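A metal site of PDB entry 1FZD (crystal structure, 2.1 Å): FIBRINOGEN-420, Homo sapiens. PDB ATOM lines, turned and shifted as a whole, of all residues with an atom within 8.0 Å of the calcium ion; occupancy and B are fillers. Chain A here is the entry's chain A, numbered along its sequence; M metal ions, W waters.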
ATOM      1  N   SER A 121     -16.320 -30.824 -25.806  1.00  0.00           N
ATOM      2  CA  SER A 121     -17.522 -31.042 -25.033  1.00  0.00           C
ATOM      3  C   SER A 121     -18.792 -30.682 -25.806  1.00  0.00           C
ATOM      4  O   SER A 121     -18.740 -29.680 -26.560  1.00  0.00           O
ATOM      5  CB  SER A 121     -17.646 -30.263 -23.736  1.00  0.00           C
ATOM      6  OG  SER A 121     -16.614 -30.517 -22.816  1.00  0.00           O
ATOM      7  N   ARG A 125     -22.309 -34.222 -23.323  1.00  0.00           N
ATOM      8  CA  ARG A 125     -21.088 -34.841 -22.935  1.00  0.00           C
ATOM      9  C   ARG A 125     -20.124 -33.750 -22.511  1.00  0.00           C
ATOM     10  O   ARG A 125     -19.201 -33.356 -23.210  1.00  0.00           O
ATOM     11  CB  ARG A 125     -20.519 -35.773 -24.016  1.00  0.00           C
ATOM     12  CG  ARG A 125     -19.462 -36.710 -23.356  1.00  0.00           C
ATOM     13  CD  ARG A 125     -18.912 -37.730 -24.334  1.00  0.00           C
ATOM     14  NE  ARG A 125     -17.497 -37.812 -24.260  1.00  0.00           N
ATOM     15  CZ  ARG A 125     -16.218 -37.809 -24.144  1.00  0.00           C
ATOM     16  NH1 ARG A 125     -15.506 -36.814 -23.528  1.00  0.00           N
ATOM     17  NH2 ARG A 125     -15.451 -38.780 -24.648  1.00  0.00           N
ATOM     18  N   ASP A 126     -20.281 -33.331 -21.299  1.00  0.00           N
ATOM     19  CA  ASP A 126     -19.514 -32.244 -20.662  1.00  0.00           C
ATOM     20  C   ASP A 126     -18.262 -32.769 -20.011  1.00  0.00           C
ATOM     21  O   ASP A 126     -18.305 -33.526 -19.042  1.00  0.00           O
ATOM     22  CB  ASP A 126     -20.459 -31.577 -19.628  1.00  0.00           C
ATOM     23  CG  ASP A 126     -19.814 -30.567 -18.716  1.00  0.00           C
ATOM     24  OD1 ASP A 126     -18.588 -30.338 -18.882  1.00  0.00           O
ATOM     25  OD2 ASP A 126     -20.439 -29.979 -17.797  1.00  0.00           O
ATOM     26  N   ALA A 127     -17.113 -32.382 -20.531  1.00  0.00           N
ATOM     27  CA  ALA A 127     -15.822 -32.738 -19.957  1.00  0.00           C
ATOM     28  C   ALA A 127     -15.076 -31.409 -19.769  1.00  0.00           C
ATOM     29  O   ALA A 127     -13.853 -31.460 -19.826  1.00  0.00           O
ATOM     30  CB  ALA A 127     -15.100 -33.732 -20.862  1.00  0.00           C
ATOM     31  N   ASP A 128     -15.799 -30.296 -19.551  1.00  0.00           N
ATOM     32  CA  ASP A 128     -14.990 -29.044 -19.421  1.00  0.00           C
ATOM     33  C   ASP A 128     -14.484 -28.854 -18.010  1.00  0.00           C
ATOM     34  O   ASP A 128     -14.717 -29.718 -17.123  1.00  0.00           O
ATOM     35  CB  ASP A 128     -15.851 -27.855 -19.904  1.00  0.00           C
ATOM     36  CG  ASP A 128     -17.105 -27.678 -19.044  1.00  0.00           C
ATOM     37  OD1 ASP A 128     -17.103 -27.818 -17.811  1.00  0.00           O
ATOM     38  OD2 ASP A 128     -18.116 -27.403 -19.647  1.00  0.00           O
ATOM     39  N   GLN A 129     -13.890 -27.686 -17.674  1.00  0.00           N
ATOM     40  CA  GLN A 129     -13.378 -27.474 -16.351  1.00  0.00           C
ATOM     41  C   GLN A 129     -14.356 -26.715 -15.444  1.00  0.00           C
ATOM     42  O   GLN A 129     -13.945 -26.215 -14.399  1.00  0.00           O
ATOM     43  CB  GLN A 129     -12.061 -26.689 -16.338  1.00  0.00           C
ATOM     44  CG  GLN A 129     -11.008 -27.130 -17.340  1.00  0.00           C
ATOM     45  CD  GLN A 129     -10.489 -28.529 -17.003  1.00  0.00           C
ATOM     46  OE1 GLN A 129      -9.552 -28.676 -16.202  1.00  0.00           O
ATOM     47  NE2 GLN A 129     -11.078 -29.530 -17.603  1.00  0.00           N
ATOM     48  N   TRP A 130     -15.621 -26.544 -15.866  1.00  0.00           N
ATOM     49  CA  TRP A 130     -16.523 -25.748 -15.066  1.00  0.00           C
ATOM     50  C   TRP A 130     -17.409 -26.712 -14.269  1.00  0.00           C
ATOM     51  O   TRP A 130     -17.843 -27.701 -14.880  1.00  0.00           O
ATOM     52  CB  TRP A 130     -17.427 -24.934 -15.992  1.00  0.00           C
ATOM     53  CG  TRP A 130     -18.300 -23.872 -15.373  1.00  0.00           C
ATOM     54  CD1 TRP A 130     -18.136 -23.233 -14.152  1.00  0.00           C
ATOM     55  CD2 TRP A 130     -19.475 -23.291 -15.987  1.00  0.00           C
ATOM     56  NE1 TRP A 130     -19.155 -22.286 -14.004  1.00  0.00           N
ATOM     57  CE2 TRP A 130     -19.986 -22.310 -15.099  1.00  0.00           C
ATOM     58  CE3 TRP A 130     -20.143 -23.529 -17.165  1.00  0.00           C
ATOM     59  CZ2 TRP A 130     -21.121 -21.569 -15.376  1.00  0.00           C
ATOM     60  CZ3 TRP A 130     -21.281 -22.780 -17.483  1.00  0.00           C
ATOM     61  CH2 TRP A 130     -21.741 -21.780 -16.589  1.00  0.00           C
ATOM     62  N   GLU A 131     -17.744 -26.310 -13.066  1.00  0.00           N
ATOM     63  CA  GLU A 131     -18.802 -27.026 -12.342  1.00  0.00           C
ATOM     64  C   GLU A 131     -20.109 -26.992 -13.118  1.00  0.00           C
ATOM     65  O   GLU A 131     -20.821 -27.943 -12.892  1.00  0.00           O
ATOM     66  CB  GLU A 131     -18.983 -26.591 -10.900  1.00  0.00           C
ATOM     67  CG  GLU A 131     -20.124 -25.616 -10.704  1.00  0.00           C
ATOM     68  CD  GLU A 131     -19.689 -24.203 -10.379  1.00  0.00           C
ATOM     69  OE1 GLU A 131     -18.485 -23.889 -10.579  1.00  0.00           O
ATOM     70  OE2 GLU A 131     -20.549 -23.402  -9.915  1.00  0.00           O
ATOM     71  N   GLU A 132     -20.378 -26.076 -14.050  1.00  0.00           N
ATOM     72  CA  GLU A 132     -21.632 -26.231 -14.817  1.00  0.00           C
ATOM     73  C   GLU A 132     -21.358 -26.721 -16.239  1.00  0.00           C
ATOM     74  O   GLU A 132     -20.244 -27.170 -16.492  1.00  0.00           O
ATOM     75  CB  GLU A 132     -22.411 -24.916 -14.979  1.00  0.00           C
ATOM     76  CG  GLU A 132     -23.810 -25.120 -14.377  1.00  0.00           C
ATOM     77  CD  GLU A 132     -23.616 -24.405 -13.021  1.00  0.00           C
ATOM     78  OE1 GLU A 132     -22.783 -24.976 -12.284  1.00  0.00           O
ATOM     79  OE2 GLU A 132     -24.240 -23.325 -12.872  1.00  0.00           O
ATOM     80  N   ASN A 133     -22.300 -26.564 -17.161  1.00  0.00           N
ATOM     81  CA  ASN A 133     -22.176 -27.058 -18.526  1.00  0.00           C
ATOM     82  C   ASN A 133     -21.926 -25.968 -19.563  1.00  0.00           C
ATOM     83  O   ASN A 133     -22.866 -25.346 -20.052  1.00  0.00           O
ATOM     84  CB  ASN A 133     -23.460 -27.837 -18.821  1.00  0.00           C
ATOM     85  CG  ASN A 133     -23.387 -28.635 -20.123  1.00  0.00           C
ATOM     86  OD1 ASN A 133     -22.579 -28.431 -21.057  1.00  0.00           O
ATOM     87  ND2 ASN A 133     -24.132 -29.744 -20.164  1.00  0.00           N
ATOM     88  N   CYS A 134     -20.662 -25.712 -19.914  1.00  0.00           N
ATOM     89  CA  CYS A 134     -20.251 -24.731 -20.892  1.00  0.00           C
ATOM     90  C   CYS A 134     -21.017 -24.872 -22.218  1.00  0.00           C
ATOM     91  O   CYS A 134     -21.503 -23.886 -22.802  1.00  0.00           O
ATOM     92  CB  CYS A 134     -18.737 -24.750 -21.231  1.00  0.00           C
ATOM     93  SG  CYS A 134     -17.563 -24.265 -19.972  1.00  0.00           S
ATOM     94  N   ALA A 135     -21.013 -26.067 -22.803  1.00  0.00           N
ATOM     95  CA  ALA A 135     -21.629 -26.240 -24.116  1.00  0.00           C
ATOM     96  C   ALA A 135     -23.127 -25.941 -24.092  1.00  0.00           C
ATOM     97  O   ALA A 135     -23.714 -25.549 -25.074  1.00  0.00           O
ATOM     98  CB  ALA A 135     -21.460 -27.698 -24.564  1.00  0.00           C
ATOM     99  N   TYR A 144     -13.900 -26.510 -24.755  1.00  0.00           N
ATOM    100  CA  TYR A 144     -14.056 -25.595 -23.660  1.00  0.00           C
ATOM    101  C   TYR A 144     -13.155 -25.836 -22.442  1.00  0.00           C
ATOM    102  O   TYR A 144     -12.785 -26.978 -22.098  1.00  0.00           O
ATOM    103  CB  TYR A 144     -15.516 -25.763 -23.174  1.00  0.00           C
ATOM    104  CG  TYR A 144     -16.603 -25.259 -24.068  1.00  0.00           C
ATOM    105  CD1 TYR A 144     -16.779 -23.879 -24.321  1.00  0.00           C
ATOM    106  CD2 TYR A 144     -17.480 -26.175 -24.650  1.00  0.00           C
ATOM    107  CE1 TYR A 144     -17.844 -23.455 -25.124  1.00  0.00           C
ATOM    108  CE2 TYR A 144     -18.517 -25.752 -25.455  1.00  0.00           C
ATOM    109  CZ  TYR A 144     -18.683 -24.376 -25.680  1.00  0.00           C
ATOM    110  OH  TYR A 144     -19.749 -24.026 -26.481  1.00  0.00           O
ATOM    111  N   ASN A 145     -12.817 -24.722 -21.823  1.00  0.00           N
ATOM    112  CA  ASN A 145     -12.046 -24.754 -20.547  1.00  0.00           C
ATOM    113  C   ASN A 145     -12.999 -24.221 -19.493  1.00  0.00           C
ATOM    114  O   ASN A 145     -13.878 -24.983 -19.014  1.00  0.00           O
ATOM    115  CB  ASN A 145     -10.727 -23.992 -20.702  1.00  0.00           C
ATOM    116  CG  ASN A 145      -9.852 -23.918 -19.474  1.00  0.00           C
ATOM    117  OD1 ASN A 145     -10.266 -24.119 -18.328  1.00  0.00           O
ATOM    118  ND2 ASN A 145      -8.584 -23.517 -19.560  1.00  0.00           N
ATOM    119  N   ASN A 146     -12.983 -22.905 -19.202  1.00  0.00           N
ATOM    120  CA  ASN A 146     -13.967 -22.352 -18.238  1.00  0.00           C
ATOM    121  C   ASN A 146     -14.237 -20.860 -18.535  1.00  0.00           C
ATOM    122  O   ASN A 146     -13.891 -19.992 -17.726  1.00  0.00           O
ATOM    123  CB  ASN A 146     -13.419 -22.560 -16.814  1.00  0.00           C
ATOM    124  CG  ASN A 146     -14.340 -22.255 -15.667  1.00  0.00           C
ATOM    125  OD1 ASN A 146     -15.529 -22.019 -15.733  1.00  0.00           O
ATOM    126  ND2 ASN A 146     -13.862 -22.243 -14.412  1.00  0.00           N
ATOM    127  N   CYS A 147     -14.841 -20.536 -19.659  1.00  0.00           N
ATOM    128  CA  CYS A 147     -15.274 -21.532 -20.653  1.00  0.00           C
ATOM    129  C   CYS A 147     -14.547 -21.275 -21.950  1.00  0.00           C
ATOM    130  O   CYS A 147     -14.092 -22.242 -22.577  1.00  0.00           O
ATOM    131  CB  CYS A 147     -16.771 -21.455 -20.898  1.00  0.00           C
ATOM    132  SG  CYS A 147     -17.855 -22.215 -19.688  1.00  0.00           S
HETATM  133 CA    CA M   1     -18.764 -28.969 -16.636  1.00  0.00          CA
HETATM  134  O   HOH W   1     -17.127 -30.717 -16.008  1.00  0.00           O
HETATM  135  O   HOH W   2     -19.990 -30.117 -14.742  1.00  0.00           O
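N of Cys 134 sits at hydrogen-bond distance from OD2 of Asp 128 (3.1 Å).
The backbone NH of Asp 128 is in hydrogen-bond range of the side-chain hydroxyl of Ser 121 (3.4 Å).
The side-chain sulfur (SG) of Cys 134 forms a disulfide with the side-chain sulfur (SG) of Cys 147.
The calcium ion is bound by the side-chain carboxylate (OD2) of Asp 126 (2.3 Å), the backbone carbonyl oxygen (O) of Glu 132 (2.3 Å), the side-chain carboxylate (OD1) of Asp 128 (2.3 Å), the backbone carbonyl oxygen (O) of Trp 130 (2.4 Å), water W1 (2.5 Å), water W2 (2.5 Å) and the side-chain carboxylate (OD1) of Asp 126 (2.6 Å).
Within 4 Å of the calcium ion: Asp 126, Asp 128, Trp 130 and Glu 132.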
